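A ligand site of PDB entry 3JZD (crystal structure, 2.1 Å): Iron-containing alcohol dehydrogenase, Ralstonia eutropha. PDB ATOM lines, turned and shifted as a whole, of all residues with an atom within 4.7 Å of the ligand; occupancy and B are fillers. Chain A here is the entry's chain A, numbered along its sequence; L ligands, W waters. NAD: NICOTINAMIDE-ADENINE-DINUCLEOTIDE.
Water W8 lies within hydrogen-bond range of a nitrogen (N1A) of the ligand (2.7 Å) and the side-chain carboxylate of Glu 50 (3.2 Å). Water W7 bridges an oxygen (O1N) of the ligand (2.7 Å) and the backbone NH (N) of Ala 258 (3.1 Å). Water W2 lies within hydrogen-bond range of ND2 of Asn 174 (2.7 Å) and O1N of the ligand (2.8 Å). Water W1 bridges an oxygen (O2A) of the ligand and the side-chain sulfur (SD) of Met 71. Water W9 lies within hydrogen-bond range of ND2 of Asn 46 (2.7 Å) and O3B of the ligand (3.0 Å). Water W5 bridges O of Gly 99 and OG of Ser 126.
Gly 98 touches the ligand (C to O1A, 3.3 Å). Lys 106 touches the ligand (NZ to N7N, 3.7 Å). Ala 124 touches the ligand. OG of Ser 126 touches C7N of the ligand, at 3.5 Å. Thr 160 touches the ligand (CA to N6A, 3.9 Å). Gly 162 touches the ligand. Leu 163 touches the ligand. CD2 of Leu 167 touches O4B of the ligand, 3.4 Å away. Leu 234 touches the ligand (CD2 to O7N, 3.7 Å). CE1 of His 257 touches C2D of the ligand, 3.5 Å away. Hydrophobic or aromatic side chains that line the ligand: His 72, Ala 124, Val 131, Leu 163, Leu 167, Leu 234 and His 257. The nearest printed residue that does not touch the ligand is Glu 50 (4.1 Å).
The side-chain amino group (NZ) of Lys 106 is in hydrogen-bond range of the side-chain hydroxyl (OG1) of Thr 129, at 2.8 Å. A ring nitrogen (ND1) of His 72 lies within hydrogen-bond range of the side-chain amino group (NZ) of Lys 140, at 2.8 Å. The side-chain hydroxyl (OG1) of Thr 44 is in hydrogen-bond range of the backbone NH (N) of Gln 47 (3.4 Å). N of Asn 46 sits close to OG1 of Thr 44. The side-chain hydroxyl (OG1) of Thr 121 sits at hydrogen-bond distance from the backbone NH (N) of Gly 98 (3.4 Å). The side-chain amide nitrogen (NE2) of Gln 47 sits close to the side-chain carboxylate (OE2) of Glu 50 (3.2 Å). The backbone carbonyl oxygen (O) of Val 131 sits at hydrogen-bond distance from the side-chain amino group (NZ) of Lys 106 (2.6 Å). A ring nitrogen (NE2) of His 257 sits at hydrogen-bond distance from the side-chain amide nitrogen of Asn 174.
O1A of the ligand sits at hydrogen-bond distance from N of Ser 100, at 2.9 Å. An oxygen (O2A) of the ligand lies within hydrogen-bond range of the side-chain hydroxyl (OG) of Ser 100, at 2.5 Å. An oxygen (O2N) of the ligand sits at hydrogen-bond distance from the side-chain hydroxyl (OG1) of Thr 122. O7N of the ligand is in hydrogen-bond range of OG1 of Thr 129 (2.7 Å). The side-chain amino group (NZ) of Lys 140 sits at hydrogen-bond distance from an oxygen (O2D) of the ligand. OG1 of Thr 44 lies within hydrogen-bond range of O2B of the ligand (2.7 Å). The backbone carbonyl oxygen (O) of Thr 121 lies within hydrogen-bond range of a nitrogen (N6A) of the ligand. The side-chain hydroxyl (OG1) of Thr 121 is in hydrogen-bond range of a nitrogen (N7A) of the ligand. OE1 of Gln 47 lies within hydrogen-bond range of O2B of the ligand. N of Gly 99 lies within hydrogen-bond range of O2N of the ligand, at 2.8 Å. N7N of the ligand lies within hydrogen-bond range of O of Val 131 (2.9 Å). ND1 of His 72 sits at hydrogen-bond distance from O3D of the ligand (2.9 Å). N6A of the ligand lies within hydrogen-bond range of O of Leu 159 (3.1 Å). An oxygen (O3B) of the ligand sits at hydrogen-bond distance from the side-chain amide nitrogen (ND2) of Asn 46.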
ATOM      1  N   THR A  44     -28.252  21.756 -30.618  1.00  0.00           N
ATOM      2  CA  THR A  44     -29.192  21.596 -29.529  1.00  0.00           C
ATOM      3  C   THR A  44     -30.582  21.553 -30.225  1.00  0.00           C
ATOM      4  O   THR A  44     -30.698  21.955 -31.387  1.00  0.00           O
ATOM      5  CB  THR A  44     -29.197  22.795 -28.583  1.00  0.00           C
ATOM      6  OG1 THR A  44     -29.498  23.976 -29.328  1.00  0.00           O
ATOM      7  CG2 THR A  44     -27.863  22.988 -27.908  1.00  0.00           C
ATOM      8  N   ASN A  46     -32.892  23.537 -29.918  1.00  0.00           N
ATOM      9  CA  ASN A  46     -33.249  24.929 -30.218  1.00  0.00           C
ATOM     10  C   ASN A  46     -32.593  25.487 -31.460  1.00  0.00           C
ATOM     11  O   ASN A  46     -32.990  26.553 -31.907  1.00  0.00           O
ATOM     12  CB  ASN A  46     -32.817  25.863 -29.081  1.00  0.00           C
ATOM     13  CG  ASN A  46     -33.585  25.660 -27.812  1.00  0.00           C
ATOM     14  OD1 ASN A  46     -34.701  25.137 -27.806  1.00  0.00           O
ATOM     15  ND2 ASN A  46     -33.000  26.121 -26.717  1.00  0.00           N
ATOM     16  N   GLN A  47     -31.552  24.829 -31.959  1.00  0.00           N
ATOM     17  CA  GLN A  47     -30.869  25.328 -33.152  1.00  0.00           C
ATOM     18  C   GLN A  47     -30.991  24.375 -34.322  1.00  0.00           C
ATOM     19  O   GLN A  47     -30.113  24.316 -35.161  1.00  0.00           O
ATOM     20  CB  GLN A  47     -29.401  25.696 -32.832  1.00  0.00           C
ATOM     21  CG  GLN A  47     -29.273  27.049 -32.123  1.00  0.00           C
ATOM     22  CD  GLN A  47     -27.855  27.382 -31.696  1.00  0.00           C
ATOM     23  OE1 GLN A  47     -27.269  26.731 -30.791  1.00  0.00           O
ATOM     24  NE2 GLN A  47     -27.300  28.426 -32.307  1.00  0.00           N
ATOM     25  N   GLU A  50     -30.790  26.215 -37.949  1.00  0.00           N
ATOM     26  CA  GLU A  50     -29.435  26.531 -38.427  1.00  0.00           C
ATOM     27  C   GLU A  50     -28.772  25.250 -38.882  1.00  0.00           C
ATOM     28  O   GLU A  50     -28.178  25.203 -39.946  1.00  0.00           O
ATOM     29  CB  GLU A  50     -28.561  27.149 -37.328  1.00  0.00           C
ATOM     30  CG  GLU A  50     -28.984  28.497 -36.830  1.00  0.00           C
ATOM     31  CD  GLU A  50     -29.890  28.447 -35.570  1.00  0.00           C
ATOM     32  OE1 GLU A  50     -31.022  27.904 -35.647  1.00  0.00           O
ATOM     33  OE2 GLU A  50     -29.453  29.050 -34.532  1.00  0.00           O
ATOM     34  N   MET A  71     -26.421  21.152 -22.494  1.00  0.00           N
ATOM     35  CA  MET A  71     -25.528  21.870 -21.583  1.00  0.00           C
ATOM     36  C   MET A  71     -24.612  20.885 -20.835  1.00  0.00           C
ATOM     37  O   MET A  71     -25.044  19.842 -20.370  1.00  0.00           O
ATOM     38  CB  MET A  71     -26.346  22.715 -20.588  1.00  0.00           C
ATOM     39  CG  MET A  71     -25.586  23.829 -19.859  1.00  0.00           C
ATOM     40  SD  MET A  71     -26.762  24.935 -18.713  1.00  0.00           S
ATOM     41  CE  MET A  71     -25.602  26.515 -18.440  1.00  0.00           C
ATOM     42  N   HIS A  72     -23.325  21.249 -20.756  1.00  0.00           N
ATOM     43  CA  HIS A  72     -22.265  20.463 -20.045  1.00  0.00           C
ATOM     44  C   HIS A  72     -22.066  18.984 -20.445  1.00  0.00           C
ATOM     45  O   HIS A  72     -21.446  18.195 -19.688  1.00  0.00           O
ATOM     46  CB  HIS A  72     -22.391  20.610 -18.504  1.00  0.00           C
ATOM     47  CG  HIS A  72     -22.295  22.031 -18.017  1.00  0.00           C
ATOM     48  ND1 HIS A  72     -21.131  22.777 -18.096  1.00  0.00           N
ATOM     49  CD2 HIS A  72     -23.207  22.821 -17.394  1.00  0.00           C
ATOM     50  CE1 HIS A  72     -21.337  23.971 -17.570  1.00  0.00           C
ATOM     51  NE2 HIS A  72     -22.588  24.027 -17.132  1.00  0.00           N
ATOM     52  N   GLY A  98     -23.268  26.904 -29.678  1.00  0.00           N
ATOM     53  CA  GLY A  98     -22.325  27.429 -28.699  1.00  0.00           C
ATOM     54  C   GLY A  98     -21.471  26.338 -28.068  1.00  0.00           C
ATOM     55  O   GLY A  98     -21.366  25.217 -28.574  1.00  0.00           O
ATOM     56  N   GLY A  99     -20.865  26.691 -26.930  1.00  0.00           N
ATOM     57  CA  GLY A  99     -20.004  25.817 -26.151  1.00  0.00           C
ATOM     58  C   GLY A  99     -20.523  24.421 -25.918  1.00  0.00           C
ATOM     59  O   GLY A  99     -19.741  23.454 -25.960  1.00  0.00           O
ATOM     60  N   SER A 100     -21.823  24.264 -25.675  1.00  0.00           N
ATOM     61  CA  SER A 100     -22.367  22.922 -25.458  1.00  0.00           C
ATOM     62  C   SER A 100     -22.382  22.029 -26.701  1.00  0.00           C
ATOM     63  O   SER A 100     -22.295  20.783 -26.611  1.00  0.00           O
ATOM     64  CB  SER A 100     -23.787  22.987 -24.869  1.00  0.00           C
ATOM     65  OG  SER A 100     -23.798  23.788 -23.697  1.00  0.00           O
ATOM     66  N   THR A 101     -22.544  22.648 -27.854  1.00  0.00           N
ATOM     67  CA  THR A 101     -22.590  21.897 -29.108  1.00  0.00           C
ATOM     68  C   THR A 101     -21.144  21.528 -29.506  1.00  0.00           C
ATOM     69  O   THR A 101     -20.856  20.386 -29.890  1.00  0.00           O
ATOM     70  CB  THR A 101     -23.340  22.679 -30.162  1.00  0.00           C
ATOM     71  OG1 THR A 101     -24.662  22.947 -29.650  1.00  0.00           O
ATOM     72  CG2 THR A 101     -23.457  21.914 -31.488  1.00  0.00           C
ATOM     73  N   LYS A 106     -16.610  17.577 -29.390  1.00  0.00           N
ATOM     74  CA  LYS A 106     -15.347  17.227 -28.719  1.00  0.00           C
ATOM     75  C   LYS A 106     -15.438  15.836 -28.128  1.00  0.00           C
ATOM     76  O   LYS A 106     -14.458  15.102 -28.174  1.00  0.00           O
ATOM     77  CB  LYS A 106     -14.982  18.235 -27.613  1.00  0.00           C
ATOM     78  CG  LYS A 106     -14.529  19.591 -28.132  1.00  0.00           C
ATOM     79  CD  LYS A 106     -14.036  20.508 -27.027  1.00  0.00           C
ATOM     80  CE  LYS A 106     -13.295  21.734 -27.543  1.00  0.00           C
ATOM     81  NZ  LYS A 106     -12.756  22.586 -26.425  1.00  0.00           N
ATOM     82  N   THR A 121     -21.719  29.946 -32.421  1.00  0.00           N
ATOM     83  CA  THR A 121     -22.810  30.887 -32.434  1.00  0.00           C
ATOM     84  C   THR A 121     -22.904  31.656 -31.082  1.00  0.00           C
ATOM     85  O   THR A 121     -23.867  32.400 -30.857  1.00  0.00           O
ATOM     86  CB  THR A 121     -24.098  30.174 -32.808  1.00  0.00           C
ATOM     87  OG1 THR A 121     -24.460  29.278 -31.780  1.00  0.00           O
ATOM     88  CG2 THR A 121     -23.917  29.397 -34.150  1.00  0.00           C
ATOM     89  N   THR A 122     -21.904  31.477 -30.209  1.00  0.00           N
ATOM     90  CA  THR A 122     -21.788  32.238 -28.991  1.00  0.00           C
ATOM     91  C   THR A 122     -20.351  32.722 -28.877  1.00  0.00           C
ATOM     92  O   THR A 122     -19.568  32.574 -29.834  1.00  0.00           O
ATOM     93  CB  THR A 122     -22.183  31.484 -27.707  1.00  0.00           C
ATOM     94  OG1 THR A 122     -21.164  30.538 -27.345  1.00  0.00           O
ATOM     95  CG2 THR A 122     -23.568  30.791 -27.880  1.00  0.00           C
ATOM     96  N   ALA A 124     -18.309  31.780 -26.268  1.00  0.00           N
ATOM     97  CA  ALA A 124     -17.698  30.863 -25.309  1.00  0.00           C
ATOM     98  C   ALA A 124     -16.222  30.549 -25.595  1.00  0.00           C
ATOM     99  O   ALA A 124     -15.476  30.381 -24.636  1.00  0.00           O
ATOM    100  CB  ALA A 124     -18.532  29.532 -25.213  1.00  0.00           C
ATOM    101  N   SER A 126     -14.744  27.817 -26.856  1.00  0.00           N
ATOM    102  CA  SER A 126     -14.410  26.407 -26.770  1.00  0.00           C
ATOM    103  C   SER A 126     -13.819  25.843 -28.089  1.00  0.00           C
ATOM    104  O   SER A 126     -13.043  24.891 -28.078  1.00  0.00           O
ATOM    105  CB  SER A 126     -15.647  25.605 -26.380  1.00  0.00           C
ATOM    106  OG  SER A 126     -15.308  24.241 -26.310  1.00  0.00           O
ATOM    107  N   THR A 129      -9.930  25.468 -27.983  1.00  0.00           N
ATOM    108  CA  THR A 129      -9.217  24.894 -26.841  1.00  0.00           C
ATOM    109  C   THR A 129      -9.224  23.397 -26.967  1.00  0.00           C
ATOM    110  O   THR A 129     -10.162  22.827 -27.519  1.00  0.00           O
ATOM    111  CB  THR A 129      -9.889  25.239 -25.462  1.00  0.00           C
ATOM    112  OG1 THR A 129     -10.934  24.284 -25.193  1.00  0.00           O
ATOM    113  CG2 THR A 129     -10.452  26.710 -25.449  1.00  0.00           C
ATOM    114  N   VAL A 131      -9.567  21.444 -24.476  1.00  0.00           N
ATOM    115  CA  VAL A 131     -10.244  20.998 -23.255  1.00  0.00           C
ATOM    116  C   VAL A 131     -11.649  20.533 -23.527  1.00  0.00           C
ATOM    117  O   VAL A 131     -12.447  21.213 -24.210  1.00  0.00           O
ATOM    118  CB  VAL A 131     -10.251  22.100 -22.166  1.00  0.00           C
ATOM    119  CG1 VAL A 131     -11.094  21.663 -20.976  1.00  0.00           C
ATOM    120  CG2 VAL A 131      -8.789  22.370 -21.695  1.00  0.00           C
ATOM    121  N   TYR A 132     -11.955  19.332 -23.047  1.00  0.00           N
ATOM    122  CA  TYR A 132     -13.298  18.770 -23.184  1.00  0.00           C
ATOM    123  C   TYR A 132     -13.899  18.616 -21.794  1.00  0.00           C
ATOM    124  O   TYR A 132     -13.190  18.618 -20.782  1.00  0.00           O
ATOM    125  CB  TYR A 132     -13.277  17.407 -23.879  1.00  0.00           C
ATOM    126  CG  TYR A 132     -12.459  16.376 -23.161  1.00  0.00           C
ATOM    127  CD1 TYR A 132     -13.033  15.554 -22.176  1.00  0.00           C
ATOM    128  CD2 TYR A 132     -11.119  16.219 -23.433  1.00  0.00           C
ATOM    129  CE1 TYR A 132     -12.274  14.634 -21.504  1.00  0.00           C
ATOM    130  CE2 TYR A 132     -10.360  15.286 -22.773  1.00  0.00           C
ATOM    131  CZ  TYR A 132     -10.938  14.505 -21.808  1.00  0.00           C
ATOM    132  OH  TYR A 132     -10.168  13.587 -21.164  1.00  0.00           O
ATOM    133  N   LYS A 140     -19.143  17.451 -13.433  1.00  0.00           N
ATOM    134  CA  LYS A 140     -18.422  17.657 -14.655  1.00  0.00           C
ATOM    135  C   LYS A 140     -16.963  17.320 -14.520  1.00  0.00           C
ATOM    136  O   LYS A 140     -16.252  17.842 -13.661  1.00  0.00           O
ATOM    137  CB  LYS A 140     -18.552  19.111 -15.078  1.00  0.00           C
ATOM    138  CG  LYS A 140     -18.040  19.363 -16.484  1.00  0.00           C
ATOM    139  CD  LYS A 140     -18.342  20.786 -16.869  1.00  0.00           C
ATOM    140  CE  LYS A 140     -17.913  21.063 -18.261  1.00  0.00           C
ATOM    141  NZ  LYS A 140     -18.454  22.368 -18.649  1.00  0.00           N
ATOM    142  N   LEU A 159     -24.768  34.127 -38.198  1.00  0.00           N
ATOM    143  CA  LEU A 159     -25.347  33.116 -37.315  1.00  0.00           C
ATOM    144  C   LEU A 159     -25.437  33.593 -35.854  1.00  0.00           C
ATOM    145  O   LEU A 159     -25.966  32.889 -35.025  1.00  0.00           O
ATOM    146  CB  LEU A 159     -24.600  31.768 -37.409  1.00  0.00           C
ATOM    147  CG  LEU A 159     -24.529  31.089 -38.775  1.00  0.00           C
ATOM    148  CD1 LEU A 159     -23.990  29.642 -38.677  1.00  0.00           C
ATOM    149  CD2 LEU A 159     -25.834  31.098 -39.509  1.00  0.00           C
ATOM    150  N   THR A 160     -24.895  34.764 -35.537  1.00  0.00           N
ATOM    151  CA  THR A 160     -24.999  35.298 -34.184  1.00  0.00           C
ATOM    152  C   THR A 160     -26.007  36.433 -34.109  1.00  0.00           C
ATOM    153  O   THR A 160     -26.282  36.918 -33.040  1.00  0.00           O
ATOM    154  CB  THR A 160     -23.634  35.788 -33.647  1.00  0.00           C
ATOM    155  OG1 THR A 160     -23.152  36.859 -34.445  1.00  0.00           O
ATOM    156  CG2 THR A 160     -22.641  34.701 -33.725  1.00  0.00           C
ATOM    157  N   GLY A 162     -29.233  36.424 -34.301  1.00  0.00           N
ATOM    158  CA  GLY A 162     -30.312  36.008 -33.457  1.00  0.00           C
ATOM    159  C   GLY A 162     -29.870  35.561 -32.066  1.00  0.00           C
ATOM    160  O   GLY A 162     -30.691  35.138 -31.296  1.00  0.00           O
ATOM    161  N   LEU A 163     -28.585  35.660 -31.729  1.00  0.00           N
ATOM    162  CA  LEU A 163     -28.157  35.349 -30.376  1.00  0.00           C
ATOM    163  C   LEU A 163     -28.931  36.392 -29.531  1.00  0.00           C
ATOM    164  O   LEU A 163     -28.817  37.579 -29.774  1.00  0.00           O
ATOM    165  CB  LEU A 163     -26.659  35.552 -30.217  1.00  0.00           C
ATOM    166  CG  LEU A 163     -26.070  35.169 -28.851  1.00  0.00           C
ATOM    167  CD1 LEU A 163     -26.299  33.709 -28.565  1.00  0.00           C
ATOM    168  CD2 LEU A 163     -24.573  35.465 -28.847  1.00  0.00           C
ATOM    169  N   PRO A 164     -29.745  35.951 -28.576  1.00  0.00           N
ATOM    170  CA  PRO A 164     -30.544  36.935 -27.821  1.00  0.00           C
ATOM    171  C   PRO A 164     -29.709  37.993 -27.132  1.00  0.00           C
ATOM    172  O   PRO A 164     -28.511  37.795 -26.872  1.00  0.00           O
ATOM    173  CB  PRO A 164     -31.283  36.099 -26.781  1.00  0.00           C
ATOM    174  CG  PRO A 164     -31.316  34.713 -27.349  1.00  0.00           C
ATOM    175  CD  PRO A 164     -29.987  34.576 -28.118  1.00  0.00           C
ATOM    176  N   LEU A 167     -27.862  36.687 -23.702  1.00  0.00           N
ATOM    177  CA  LEU A 167     -26.683  35.844 -23.916  1.00  0.00           C
ATOM    178  C   LEU A 167     -25.589  36.582 -24.719  1.00  0.00           C
ATOM    179  O   LEU A 167     -24.413  36.308 -24.505  1.00  0.00           O
ATOM    180  CB  LEU A 167     -27.075  34.505 -24.552  1.00  0.00           C
ATOM    181  CG  LEU A 167     -26.036  33.396 -24.646  1.00  0.00           C
ATOM    182  CD1 LEU A 167     -25.370  33.160 -23.261  1.00  0.00           C
ATOM    183  CD2 LEU A 167     -26.723  32.073 -25.255  1.00  0.00           C
ATOM    184  N   ASN A 174     -18.100  36.247 -20.605  1.00  0.00           N
ATOM    185  CA  ASN A 174     -17.452  34.950 -20.422  1.00  0.00           C
ATOM    186  C   ASN A 174     -16.114  34.963 -21.219  1.00  0.00           C
ATOM    187  O   ASN A 174     -15.056  34.609 -20.702  1.00  0.00           O
ATOM    188  CB  ASN A 174     -18.416  33.867 -20.861  1.00  0.00           C
ATOM    189  CG  ASN A 174     -17.872  32.469 -20.759  1.00  0.00           C
ATOM    190  OD1 ASN A 174     -16.812  32.205 -20.169  1.00  0.00           O
ATOM    191  ND2 ASN A 174     -18.589  31.556 -21.348  1.00  0.00           N
ATOM    192  N   HIS A 178     -11.838  34.997 -19.947  1.00  0.00           N
ATOM    193  CA  HIS A 178     -10.691  34.154 -20.377  1.00  0.00           C
ATOM    194  C   HIS A 178      -9.447  35.031 -20.566  1.00  0.00           C
ATOM    195  O   HIS A 178      -8.349  34.726 -20.094  1.00  0.00           O
ATOM    196  CB  HIS A 178     -10.920  33.450 -21.730  1.00  0.00           C
ATOM    197  CG  HIS A 178     -12.189  32.657 -21.835  1.00  0.00           C
ATOM    198  ND1 HIS A 178     -12.774  31.988 -20.778  1.00  0.00           N
ATOM    199  CD2 HIS A 178     -12.952  32.364 -22.921  1.00  0.00           C
ATOM    200  CE1 HIS A 178     -13.851  31.349 -21.195  1.00  0.00           C
ATOM    201  NE2 HIS A 178     -13.983  31.564 -22.495  1.00  0.00           N
ATOM    202  N   LEU A 234      -7.548  31.292 -23.641  1.00  0.00           N
ATOM    203  CA  LEU A 234      -8.024  30.160 -22.802  1.00  0.00           C
ATOM    204  C   LEU A 234      -7.321  28.874 -23.199  1.00  0.00           C
ATOM    205  O   LEU A 234      -6.952  28.097 -22.365  1.00  0.00           O
ATOM    206  CB  LEU A 234      -9.551  29.997 -22.979  1.00  0.00           C
ATOM    207  CG  LEU A 234     -10.244  28.832 -22.280  1.00  0.00           C
ATOM    208  CD1 LEU A 234     -10.082  28.894 -20.743  1.00  0.00           C
ATOM    209  CD2 LEU A 234     -11.752  28.724 -22.725  1.00  0.00           C
ATOM    210  N   HIS A 257     -24.298  29.069 -17.020  1.00  0.00           N
ATOM    211  CA  HIS A 257     -22.876  29.318 -17.327  1.00  0.00           C
ATOM    212  C   HIS A 257     -22.447  30.782 -17.622  1.00  0.00           C
ATOM    213  O   HIS A 257     -21.733  31.401 -16.820  1.00  0.00           O
ATOM    214  CB  HIS A 257     -22.426  28.358 -18.462  1.00  0.00           C
ATOM    215  CG  HIS A 257     -21.023  28.562 -18.865  1.00  0.00           C
ATOM    216  ND1 HIS A 257     -19.974  27.983 -18.186  1.00  0.00           N
ATOM    217  CD2 HIS A 257     -20.477  29.324 -19.844  1.00  0.00           C
ATOM    218  CE1 HIS A 257     -18.829  28.380 -18.749  1.00  0.00           C
ATOM    219  NE2 HIS A 257     -19.119  29.176 -19.766  1.00  0.00           N
ATOM    220  N   ALA A 258     -22.863  31.334 -18.759  1.00  0.00           N
ATOM    221  CA  ALA A 258     -22.436  32.705 -19.148  1.00  0.00           C
ATOM    222  C   ALA A 258     -22.765  33.756 -18.078  1.00  0.00           C
ATOM    223  O   ALA A 258     -21.961  34.637 -17.737  1.00  0.00           O
ATOM    224  CB  ALA A 258     -23.065  33.092 -20.486  1.00  0.00           C
HETATM  225  PA  NAD L   1     -24.708  26.989 -24.770  1.00  0.00           P
HETATM  226  O1A NAD L   1     -23.922  26.267 -25.833  1.00  0.00           O
HETATM  227  O2A NAD L   1     -24.929  26.066 -23.658  1.00  0.00           O
HETATM  228  O5B NAD L   1     -25.982  27.713 -25.417  1.00  0.00           O
HETATM  229  C5B NAD L   1     -27.057  28.155 -24.593  1.00  0.00           C
HETATM  230  C4B NAD L   1     -28.331  28.225 -25.429  1.00  0.00           C
HETATM  231  O4B NAD L   1     -28.244  29.241 -26.414  1.00  0.00           O
HETATM  232  C3B NAD L   1     -28.552  26.927 -26.201  1.00  0.00           C
HETATM  233  O3B NAD L   1     -29.900  26.567 -26.175  1.00  0.00           O
HETATM  234  C2B NAD L   1     -28.207  27.269 -27.632  1.00  0.00           C
HETATM  235  O2B NAD L   1     -28.899  26.464 -28.547  1.00  0.00           O
HETATM  236  C1B NAD L   1     -28.609  28.740 -27.675  1.00  0.00           C
HETATM  237  N9A NAD L   1     -27.872  29.485 -28.701  1.00  0.00           N
HETATM  238  C8A NAD L   1     -26.506  29.461 -28.846  1.00  0.00           C
HETATM  239  N7A NAD L   1     -26.187  30.291 -29.853  1.00  0.00           N
HETATM  240  C5A NAD L   1     -27.299  30.835 -30.365  1.00  0.00           C
HETATM  241  C6A NAD L   1     -27.519  31.706 -31.447  1.00  0.00           C
HETATM  242  N6A NAD L   1     -26.563  32.440 -31.981  1.00  0.00           N
HETATM  243  N1A NAD L   1     -28.815  32.040 -31.756  1.00  0.00           N
HETATM  244  C2A NAD L   1     -29.871  31.529 -31.039  1.00  0.00           C
HETATM  245  N3A NAD L   1     -29.648  30.680 -29.966  1.00  0.00           N
HETATM  246  C4A NAD L   1     -28.374  30.313 -29.646  1.00  0.00           C
HETATM  247  O3  NAD L   1     -23.991  28.295 -24.151  1.00  0.00           O
HETATM  248  PN  NAD L   1     -22.416  28.632 -24.157  1.00  0.00           P
HETATM  249  O1N NAD L   1     -22.295  29.678 -23.056  1.00  0.00           O
HETATM  250  O2N NAD L   1     -21.960  28.879 -25.542  1.00  0.00           O
HETATM  251  O5D NAD L   1     -21.669  27.329 -23.733  1.00  0.00           O
HETATM  252  C5D NAD L   1     -21.413  27.061 -22.389  1.00  0.00           C
HETATM  253  C4D NAD L   1     -21.001  25.602 -22.298  1.00  0.00           C
HETATM  254  O4D NAD L   1     -19.788  25.481 -22.992  1.00  0.00           O
HETATM  255  C3D NAD L   1     -20.721  25.174 -20.872  1.00  0.00           C
HETATM  256  O3D NAD L   1     -20.905  23.791 -20.799  1.00  0.00           O
HETATM  257  C2D NAD L   1     -19.281  25.530 -20.702  1.00  0.00           C
HETATM  258  O2D NAD L   1     -18.692  24.835 -19.628  1.00  0.00           O
HETATM  259  C1D NAD L   1     -18.762  25.126 -22.080  1.00  0.00           C
HETATM  260  N1N NAD L   1     -17.481  25.779 -22.389  1.00  0.00           N
HETATM  261  C2N NAD L   1     -16.372  24.973 -22.551  1.00  0.00           C
HETATM  262  C3N NAD L   1     -15.138  25.546 -22.842  1.00  0.00           C
HETATM  263  C7N NAD L   1     -13.939  24.661 -23.104  1.00  0.00           C
HETATM  264  O7N NAD L   1     -12.717  25.241 -23.463  1.00  0.00           O
HETATM  265  N7N NAD L   1     -14.014  23.344 -23.060  1.00  0.00           N
HETATM  266  C4N NAD L   1     -15.040  26.932 -22.979  1.00  0.00           C
HETATM  267  C5N NAD L   1     -16.170  27.737 -22.825  1.00  0.00           C
HETATM  268  C6N NAD L   1     -17.402  27.129 -22.547  1.00  0.00           C
HETATM  269  O   HOH W   1     -24.837  27.081 -21.024  1.00  0.00           O
HETATM  270  O   HOH W   2     -20.552  31.838 -23.129  1.00  0.00           O
HETATM  271  O   HOH W   3     -16.299  25.924 -19.200  1.00  0.00           O
HETATM  272  O   HOH W   4     -25.138  25.377 -28.103  1.00  0.00           O
HETATM  273  O   HOH W   5     -17.323  22.956 -25.084  1.00  0.00           O
HETATM  274  O   HOH W   6     -11.138  25.403 -21.517  1.00  0.00           O
HETATM  275  O   HOH W   7     -24.177  29.906 -21.150  1.00  0.00           O
HETATM  276  O   HOH W   8     -29.774  32.233 -34.254  1.00  0.00           O
HETATM  277  O   HOH W   9     -31.421  23.984 -26.231  1.00  0.00           O
